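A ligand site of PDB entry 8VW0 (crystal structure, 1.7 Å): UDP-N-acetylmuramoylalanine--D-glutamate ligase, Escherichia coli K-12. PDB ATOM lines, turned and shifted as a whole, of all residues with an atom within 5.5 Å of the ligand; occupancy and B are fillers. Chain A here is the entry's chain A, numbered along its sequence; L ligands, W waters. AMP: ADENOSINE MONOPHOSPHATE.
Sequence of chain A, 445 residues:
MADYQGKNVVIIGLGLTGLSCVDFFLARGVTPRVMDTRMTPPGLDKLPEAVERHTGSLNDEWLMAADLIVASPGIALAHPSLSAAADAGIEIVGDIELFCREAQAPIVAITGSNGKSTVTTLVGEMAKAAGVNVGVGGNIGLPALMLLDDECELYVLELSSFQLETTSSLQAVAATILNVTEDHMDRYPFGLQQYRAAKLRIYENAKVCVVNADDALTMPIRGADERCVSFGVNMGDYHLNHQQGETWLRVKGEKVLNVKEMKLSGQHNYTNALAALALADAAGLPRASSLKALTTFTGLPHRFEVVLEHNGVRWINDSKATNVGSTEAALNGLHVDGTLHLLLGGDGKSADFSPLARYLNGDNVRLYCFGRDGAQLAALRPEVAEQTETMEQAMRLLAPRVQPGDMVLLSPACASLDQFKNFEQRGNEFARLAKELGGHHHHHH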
ATOM      1  N   ASN A 114     -18.514  33.483  18.367  1.00  0.00           N
ATOM      2  CA  ASN A 114     -19.101  32.203  18.728  1.00  0.00           C
ATOM      3  C   ASN A 114     -19.573  32.253  20.176  1.00  0.00           C
ATOM      4  O   ASN A 114     -18.993  32.929  21.020  1.00  0.00           O
ATOM      5  CB  ASN A 114     -18.092  31.069  18.540  1.00  0.00           C
ATOM      6  CG  ASN A 114     -17.679  30.877  17.059  1.00  0.00           C
ATOM      7  OD1 ASN A 114     -18.505  30.527  16.210  1.00  0.00           O
ATOM      8  ND2 ASN A 114     -16.399  31.110  16.763  1.00  0.00           N
ATOM      9  N   GLY A 115     -20.653  31.506  20.459  1.00  0.00           N
ATOM     10  CA  GLY A 115     -21.257  31.469  21.780  1.00  0.00           C
ATOM     11  C   GLY A 115     -22.440  32.399  21.987  1.00  0.00           C
ATOM     12  O   GLY A 115     -23.057  32.357  23.069  1.00  0.00           O
ATOM     13  N   LYS A 116     -22.772  33.240  21.009  1.00  0.00           N
ATOM     14  CA  LYS A 116     -23.834  34.220  21.225  1.00  0.00           C
ATOM     15  C   LYS A 116     -25.147  33.562  21.594  1.00  0.00           C
ATOM     16  O   LYS A 116     -25.887  34.068  22.450  1.00  0.00           O
ATOM     17  CB  LYS A 116     -24.060  35.045  19.961  1.00  0.00           C
ATOM     18  CG  LYS A 116     -22.926  35.890  19.511  1.00  0.00           C
ATOM     19  CD  LYS A 116     -23.419  36.844  18.420  1.00  0.00           C
ATOM     20  CE  LYS A 116     -23.791  36.140  17.127  1.00  0.00           C
ATOM     21  NZ  LYS A 116     -22.630  35.608  16.424  1.00  0.00           N
ATOM     22  N   SER A 117     -25.499  32.481  20.904  1.00  0.00           N
ATOM     23  CA  SER A 117     -26.805  31.878  21.141  1.00  0.00           C
ATOM     24  C   SER A 117     -26.870  31.246  22.518  1.00  0.00           C
ATOM     25  O   SER A 117     -27.869  31.376  23.237  1.00  0.00           O
ATOM     26  CB  SER A 117     -27.115  30.841  20.069  1.00  0.00           C
ATOM     27  OG  SER A 117     -27.133  31.473  18.804  1.00  0.00           O
ATOM     28  N   THR A 118     -25.788  30.580  22.938  1.00  0.00           N
ATOM     29  CA  THR A 118     -25.802  29.961  24.269  1.00  0.00           C
ATOM     30  C   THR A 118     -25.932  31.031  25.356  1.00  0.00           C
ATOM     31  O   THR A 118     -26.745  30.895  26.277  1.00  0.00           O
ATOM     32  CB  THR A 118     -24.536  29.133  24.464  1.00  0.00           C
ATOM     33  OG1 THR A 118     -24.548  28.000  23.605  1.00  0.00           O
ATOM     34  CG2 THR A 118     -24.402  28.657  25.875  1.00  0.00           C
ATOM     35  N   VAL A 119     -25.142  32.095  25.267  1.00  0.00           N
ATOM     36  CA  VAL A 119     -25.164  33.092  26.320  1.00  0.00           C
ATOM     37  C   VAL A 119     -26.487  33.829  26.328  1.00  0.00           C
ATOM     38  O   VAL A 119     -27.030  34.132  27.397  1.00  0.00           O
ATOM     39  CB  VAL A 119     -23.959  34.045  26.168  1.00  0.00           C
ATOM     40  CG1 VAL A 119     -24.067  35.205  27.145  1.00  0.00           C
ATOM     41  CG2 VAL A 119     -22.676  33.268  26.379  1.00  0.00           C
ATOM     42  N   LEU A 178     -18.226  38.538  23.223  1.00  0.00           N
ATOM     43  CA  LEU A 178     -17.732  37.328  23.891  1.00  0.00           C
ATOM     44  C   LEU A 178     -16.346  36.958  23.424  1.00  0.00           C
ATOM     45  O   LEU A 178     -15.546  36.416  24.191  1.00  0.00           O
ATOM     46  CB  LEU A 178     -18.689  36.168  23.649  1.00  0.00           C
ATOM     47  CG  LEU A 178     -20.085  36.322  24.220  1.00  0.00           C
ATOM     48  CD1 LEU A 178     -20.956  35.187  23.636  1.00  0.00           C
ATOM     49  CD2 LEU A 178     -20.021  36.265  25.737  1.00  0.00           C
ATOM     50  N   ASN A 179     -16.040  37.204  22.150  1.00  0.00           N
ATOM     51  CA  ASN A 179     -14.792  36.822  21.519  1.00  0.00           C
ATOM     52  C   ASN A 179     -14.811  37.359  20.088  1.00  0.00           C
ATOM     53  O   ASN A 179     -15.870  37.717  19.559  1.00  0.00           O
ATOM     54  CB  ASN A 179     -14.562  35.313  21.494  1.00  0.00           C
ATOM     55  CG  ASN A 179     -15.777  34.533  20.987  1.00  0.00           C
ATOM     56  OD1 ASN A 179     -16.146  34.593  19.808  1.00  0.00           O
ATOM     57  ND2 ASN A 179     -16.395  33.809  21.888  1.00  0.00           N
ATOM     58  N   HIS A 268     -15.375  26.104  27.471  1.00  0.00           N
ATOM     59  CA  HIS A 268     -15.953  27.298  26.844  1.00  0.00           C
ATOM     60  C   HIS A 268     -17.405  27.500  27.248  1.00  0.00           C
ATOM     61  O   HIS A 268     -17.869  28.642  27.329  1.00  0.00           O
ATOM     62  CB  HIS A 268     -15.804  27.236  25.330  1.00  0.00           C
ATOM     63  CG  HIS A 268     -16.479  26.057  24.704  1.00  0.00           C
ATOM     64  ND1 HIS A 268     -16.275  24.763  25.133  1.00  0.00           N
ATOM     65  CD2 HIS A 268     -17.335  25.980  23.660  1.00  0.00           C
ATOM     66  CE1 HIS A 268     -16.992  23.938  24.389  1.00  0.00           C
ATOM     67  NE2 HIS A 268     -17.637  24.660  23.477  1.00  0.00           N
ATOM     68  N   ASN A 269     -18.144  26.418  27.538  1.00  0.00           N
ATOM     69  CA  ASN A 269     -19.475  26.601  28.098  1.00  0.00           C
ATOM     70  C   ASN A 269     -19.428  27.120  29.532  1.00  0.00           C
ATOM     71  O   ASN A 269     -20.303  27.895  29.928  1.00  0.00           O
ATOM     72  CB  ASN A 269     -20.263  25.311  28.014  1.00  0.00           C
ATOM     73  CG  ASN A 269     -20.963  25.149  26.682  1.00  0.00           C
ATOM     74  OD1 ASN A 269     -21.298  26.150  26.015  1.00  0.00           O
ATOM     75  ND2 ASN A 269     -21.190  23.909  26.289  1.00  0.00           N
ATOM     76  N   THR A 271     -17.135  29.286  30.572  1.00  0.00           N
ATOM     77  CA  THR A 271     -16.936  30.725  30.439  1.00  0.00           C
ATOM     78  C   THR A 271     -18.179  31.403  29.857  1.00  0.00           C
ATOM     79  O   THR A 271     -18.464  32.540  30.208  1.00  0.00           O
ATOM     80  CB  THR A 271     -15.686  31.079  29.619  1.00  0.00           C
ATOM     81  OG1 THR A 271     -15.794  30.606  28.279  1.00  0.00           O
ATOM     82  CG2 THR A 271     -14.408  30.544  30.280  1.00  0.00           C
ATOM     83  N   ASN A 272     -18.963  30.704  29.032  1.00  0.00           N
ATOM     84  CA  ASN A 272     -20.268  31.235  28.634  1.00  0.00           C
ATOM     85  C   ASN A 272     -21.172  31.420  29.843  1.00  0.00           C
ATOM     86  O   ASN A 272     -21.881  32.426  29.950  1.00  0.00           O
ATOM     87  CB  ASN A 272     -20.966  30.301  27.650  1.00  0.00           C
ATOM     88  CG  ASN A 272     -20.329  30.319  26.305  1.00  0.00           C
ATOM     89  OD1 ASN A 272     -19.608  31.248  25.950  1.00  0.00           O
ATOM     90  ND2 ASN A 272     -20.603  29.267  25.514  1.00  0.00           N
ATOM     91  N   LEU A 300     -28.073  24.211  24.399  1.00  0.00           N
ATOM     92  CA  LEU A 300     -28.679  24.168  23.083  1.00  0.00           C
ATOM     93  C   LEU A 300     -28.213  22.925  22.335  1.00  0.00           C
ATOM     94  O   LEU A 300     -27.072  22.476  22.501  1.00  0.00           O
ATOM     95  CB  LEU A 300     -28.315  25.395  22.288  1.00  0.00           C
ATOM     96  CG  LEU A 300     -28.813  26.750  22.791  1.00  0.00           C
ATOM     97  CD1 LEU A 300     -28.334  27.877  21.872  1.00  0.00           C
ATOM     98  CD2 LEU A 300     -30.302  26.759  22.935  1.00  0.00           C
ATOM     99  N   HIS A 302     -26.494  20.699  19.677  1.00  0.00           N
ATOM    100  CA  HIS A 302     -25.375  20.799  18.721  1.00  0.00           C
ATOM    101  C   HIS A 302     -24.284  21.744  19.204  1.00  0.00           C
ATOM    102  O   HIS A 302     -23.362  22.008  18.453  1.00  0.00           O
ATOM    103  CB  HIS A 302     -25.836  21.267  17.333  1.00  0.00           C
ATOM    104  CG  HIS A 302     -27.128  20.648  16.868  1.00  0.00           C
ATOM    105  ND1 HIS A 302     -27.252  19.321  16.542  1.00  0.00           N
ATOM    106  CD2 HIS A 302     -28.346  21.200  16.657  1.00  0.00           C
ATOM    107  CE1 HIS A 302     -28.491  19.061  16.192  1.00  0.00           C
ATOM    108  NE2 HIS A 302     -29.184  20.184  16.253  1.00  0.00           N
ATOM    109  N   ARG A 303     -24.381  22.266  20.438  1.00  0.00           N
ATOM    110  CA  ARG A 303     -23.377  23.134  21.060  1.00  0.00           C
ATOM    111  C   ARG A 303     -22.625  22.356  22.137  1.00  0.00           C
ATOM    112  O   ARG A 303     -22.981  22.412  23.317  1.00  0.00           O
ATOM    113  CB  ARG A 303     -24.016  24.366  21.683  1.00  0.00           C
ATOM    114  CG  ARG A 303     -24.335  25.475  20.729  1.00  0.00           C
ATOM    115  CD  ARG A 303     -25.511  25.163  19.859  1.00  0.00           C
ATOM    116  NE  ARG A 303     -25.997  26.357  19.183  1.00  0.00           N
ATOM    117  CZ  ARG A 303     -27.104  26.413  18.452  1.00  0.00           C
ATOM    118  NH1 ARG A 303     -27.904  25.358  18.329  1.00  0.00           N
ATOM    119  NH2 ARG A 303     -27.402  27.533  17.811  1.00  0.00           N
ATOM    120  N   PHE A 304     -21.553  21.699  21.749  1.00  0.00           N
ATOM    121  CA  PHE A 304     -20.796  20.833  22.651  1.00  0.00           C
ATOM    122  C   PHE A 304     -21.749  20.055  23.560  1.00  0.00           C
ATOM    123  O   PHE A 304     -21.663  20.074  24.787  1.00  0.00           O
ATOM    124  CB  PHE A 304     -19.804  21.653  23.463  1.00  0.00           C
ATOM    125  CG  PHE A 304     -18.592  20.872  23.913  1.00  0.00           C
ATOM    126  CD1 PHE A 304     -17.506  20.733  23.079  1.00  0.00           C
ATOM    127  CD2 PHE A 304     -18.559  20.276  25.146  1.00  0.00           C
ATOM    128  CE1 PHE A 304     -16.389  20.024  23.476  1.00  0.00           C
ATOM    129  CE2 PHE A 304     -17.462  19.561  25.556  1.00  0.00           C
ATOM    130  CZ  PHE A 304     -16.369  19.431  24.712  1.00  0.00           C
ATOM    131  N   ASP A 318     -20.877  18.584  18.674  1.00  0.00           N
ATOM    132  CA  ASP A 318     -20.557  19.990  18.517  1.00  0.00           C
ATOM    133  C   ASP A 318     -20.709  20.375  17.042  1.00  0.00           C
ATOM    134  O   ASP A 318     -19.864  21.086  16.485  1.00  0.00           O
ATOM    135  CB  ASP A 318     -19.157  20.304  19.021  1.00  0.00           C
ATOM    136  CG  ASP A 318     -18.924  21.769  19.261  1.00  0.00           C
ATOM    137  OD1 ASP A 318     -19.900  22.480  19.597  1.00  0.00           O
ATOM    138  OD2 ASP A 318     -17.753  22.219  19.109  1.00  0.00           O
ATOM    139  N   SER A 319     -21.757  19.859  16.409  1.00  0.00           N
ATOM    140  CA  SER A 319     -21.959  20.125  14.996  1.00  0.00           C
ATOM    141  C   SER A 319     -22.113  21.614  14.685  1.00  0.00           C
ATOM    142  O   SER A 319     -21.881  22.013  13.547  1.00  0.00           O
ATOM    143  CB  SER A 319     -23.196  19.365  14.500  1.00  0.00           C
ATOM    144  OG  SER A 319     -23.336  19.558  13.102  1.00  0.00           O
ATOM    145  N   LYS A 320     -22.512  22.451  15.659  1.00  0.00           N
ATOM    146  CA  LYS A 320     -22.609  23.878  15.337  1.00  0.00           C
ATOM    147  C   LYS A 320     -21.227  24.507  15.160  1.00  0.00           C
ATOM    148  O   LYS A 320     -21.137  25.657  14.700  1.00  0.00           O
ATOM    149  CB  LYS A 320     -23.411  24.613  16.420  1.00  0.00           C
ATOM    150  CG  LYS A 320     -24.248  25.837  15.972  1.00  0.00           C
ATOM    151  CD  LYS A 320     -23.440  26.953  15.356  1.00  0.00           C
ATOM    152  CE  LYS A 320     -24.144  28.324  15.481  1.00  0.00           C
ATOM    153  NZ  LYS A 320     -25.149  28.544  14.424  1.00  0.00           N
ATOM    154  N   ALA A 321     -20.150  23.769  15.467  1.00  0.00           N
ATOM    155  CA  ALA A 321     -18.790  24.232  15.222  1.00  0.00           C
ATOM    156  C   ALA A 321     -18.530  24.155  13.715  1.00  0.00           C
ATOM    157  O   ALA A 321     -17.963  23.198  13.186  1.00  0.00           O
ATOM    158  CB  ALA A 321     -17.765  23.422  16.009  1.00  0.00           C
ATOM    159  N   THR A 322     -18.943  25.196  13.001  1.00  0.00           N
ATOM    160  CA  THR A 322     -18.825  25.230  11.561  1.00  0.00           C
ATOM    161  C   THR A 322     -17.600  26.012  11.091  1.00  0.00           C
ATOM    162  O   THR A 322     -17.456  26.261   9.880  1.00  0.00           O
ATOM    163  CB  THR A 322     -20.096  25.814  10.938  1.00  0.00           C
ATOM    164  OG1 THR A 322     -20.337  27.111  11.471  1.00  0.00           O
ATOM    165  CG2 THR A 322     -21.291  24.921  11.209  1.00  0.00           C
ATOM    166  N   GLY A 325     -12.624  28.785  14.681  1.00  0.00           N
ATOM    167  CA  GLY A 325     -12.664  29.366  16.013  1.00  0.00           C
ATOM    168  C   GLY A 325     -13.525  28.582  16.990  1.00  0.00           C
ATOM    169  O   GLY A 325     -13.189  28.478  18.169  1.00  0.00           O
ATOM    170  N   SER A 326     -14.629  28.016  16.501  1.00  0.00           N
ATOM    171  CA  SER A 326     -15.503  27.200  17.349  1.00  0.00           C
ATOM    172  C   SER A 326     -14.807  25.924  17.793  1.00  0.00           C
ATOM    173  O   SER A 326     -14.915  25.506  18.956  1.00  0.00           O
ATOM    174  CB  SER A 326     -16.787  26.852  16.583  1.00  0.00           C
ATOM    175  OG  SER A 326     -17.626  27.982  16.435  1.00  0.00           O
ATOM    176  N   ALA A 329     -12.009  26.613  20.331  1.00  0.00           N
ATOM    177  CA  ALA A 329     -12.527  26.794  21.685  1.00  0.00           C
ATOM    178  C   ALA A 329     -12.956  25.483  22.321  1.00  0.00           C
ATOM    179  O   ALA A 329     -12.905  25.356  23.554  1.00  0.00           O
ATOM    180  CB  ALA A 329     -13.690  27.782  21.662  1.00  0.00           C
HETATM  181  P   AMP L   1     -23.729  29.324  19.685  1.00  0.00           P
HETATM  182  O1P AMP L   1     -23.885  29.293  21.176  1.00  0.00           O
HETATM  183  O2P AMP L   1     -24.737  28.554  18.851  1.00  0.00           O
HETATM  184  O3P AMP L   1     -23.455  30.670  19.026  1.00  0.00           O
HETATM  185  O5' AMP L   1     -22.390  28.483  19.472  1.00  0.00           O
HETATM  186  C5' AMP L   1     -21.791  28.402  18.184  1.00  0.00           C
HETATM  187  C4' AMP L   1     -20.621  27.448  18.143  1.00  0.00           C
HETATM  188  O4' AMP L   1     -19.538  28.018  18.909  1.00  0.00           O
HETATM  189  C3' AMP L   1     -20.870  26.058  18.737  1.00  0.00           C
HETATM  190  O3' AMP L   1     -20.015  25.101  18.102  1.00  0.00           O
HETATM  191  C2' AMP L   1     -20.427  26.247  20.181  1.00  0.00           C
HETATM  192  O2' AMP L   1     -20.077  25.073  20.867  1.00  0.00           O
HETATM  193  C1' AMP L   1     -19.234  27.181  20.002  1.00  0.00           C
HETATM  194  N9  AMP L   1     -18.972  28.030  21.152  1.00  0.00           N
HETATM  195  C8  AMP L   1     -19.748  28.153  22.250  1.00  0.00           C
HETATM  196  N7  AMP L   1     -19.202  29.016  23.127  1.00  0.00           N
HETATM  197  C5  AMP L   1     -18.055  29.443  22.581  1.00  0.00           C
HETATM  198  C6  AMP L   1     -17.014  30.357  22.997  1.00  0.00           C
HETATM  199  N6  AMP L   1     -17.131  30.981  24.175  1.00  0.00           N
HETATM  200  N1  AMP L   1     -15.971  30.571  22.152  1.00  0.00           N
HETATM  201  C2  AMP L   1     -15.884  29.939  20.955  1.00  0.00           C
HETATM  202  N3  AMP L   1     -16.822  29.066  20.524  1.00  0.00           N
HETATM  203  C4  AMP L   1     -17.897  28.791  21.277  1.00  0.00           C
HETATM  204  O   HOH W   1     -15.916  33.570  24.942  1.00  0.00           O
HETATM  205  O   HOH W   2     -13.607  31.382  22.917  1.00  0.00           O
HETATM  206  O   HOH W   3     -17.461  32.513  26.915  1.00  0.00           O
HETATM  207  O   HOH W   4     -22.153  26.565  23.736  1.00  0.00           O
HETATM  208  O   HOH W   5     -25.336  32.440  16.924  1.00  0.00           O
HETATM  209  O   HOH W   6     -17.213  24.435  20.367  1.00  0.00           O
HETATM  210  O   HOH W   7     -22.380  32.869  17.828  1.00  0.00           O
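The backbone NH (N) of Lys 116 is in hydrogen-bond range of an oxygen (O3P) of the ligand (3.3 Å).
N of Ser 117 sits at hydrogen-bond distance from O3P of the ligand.
The side-chain amide nitrogen (ND2) of Asn 272 is in hydrogen-bond range of a nitrogen (N7) of the ligand, 2.8 Å away.
The side-chain carboxylate (OD1) of Asp 318 is in hydrogen-bond range of an oxygen (O2') of the ligand (2.9 Å).
N of Thr 118 is in hydrogen-bond range of O1P of the ligand (2.9 Å).
O4' of the ligand sits at hydrogen-bond distance from OG of Ser 326.
O1P of the ligand is in hydrogen-bond range of OG1 of Thr 118 (2.8 Å).
The backbone NH (N) of Ala 321 is in hydrogen-bond range of an oxygen (O3') of the ligand.
ND2 of Asn 179 sits at hydrogen-bond distance from N1 of the ligand.
An oxygen (O3P) of the ligand is in hydrogen-bond range of the backbone NH (N) of Gly 115, at 3.3 Å.
An oxygen (O2P) of the ligand lies within salt-bridge range of the guanidinium group (NE) of Arg 303 (2.6 Å).
The side-chain amide oxygen of Asn 114 lies within hydrogen-bond range of the side-chain hydroxyl of Ser 326.
N of Lys 320 sits at hydrogen-bond distance from O of His 302 (3.0 Å).
O of Asn 114 is in hydrogen-bond range of ND2 of Asn 179, 2.9 Å away.
N of Phe 304 is in hydrogen-bond range of OD1 of Asp 318, 2.8 Å away.
O of His 268 sits at hydrogen-bond distance from OG1 of Thr 271 (3.0 Å).
The side-chain amide nitrogen of Asn 272 lies close to the backbone carbonyl oxygen of His 268 (3.3 Å).
ND2 of Asn 272 sits at hydrogen-bond distance from OD1 of Asn 269, 3.2 Å away.
Asn 114 touches the ligand (CB to N3, 3.1 Å).
His 268 touches the ligand.
N of Phe 304 touches O2' of the ligand (3.8 Å).
C of Lys 320 touches O3' of the ligand, at 3.2 Å.
CB of Ala 329 touches C2 of the ligand, 3.2 Å away.
Hydrophobic or aromatic side chains that line the ligand: His 268, Ala 321 and Ala 329.
The nearest printed residue that does not touch the ligand is Gly 325 (4.1 Å).
Water W7 lies within hydrogen-bond range of O3P of the ligand, NZ of Lys 116 and N of Gly 115.
Water W1 lies within hydrogen-bond range of N6 of the ligand, O of Leu 178 and ND2 of Asn 179.
Water W6 lies within hydrogen-bond range of OD2 of Asp 318 (2.6 Å), O of Ser 326 (2.9 Å), O2' of the ligand (3.0 Å) and NE2 of His 268 (3.1 Å).
Water W3 lies within hydrogen-bond range of the side-chain amide oxygen (OD1) of Asn 272 (2.7 Å), the side-chain hydroxyl (OG1) of Thr 271 (2.9 Å) and a nitrogen (N6) of the ligand (3.2 Å).
Water W4 bridges OD1 of Asn 269 (2.5 Å) and OG1 of Thr 118 (2.8 Å).
Water W5 bridges the side-chain hydroxyl of Ser 117 (2.8 Å) and an oxygen (O3P) of the ligand (3.3 Å).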
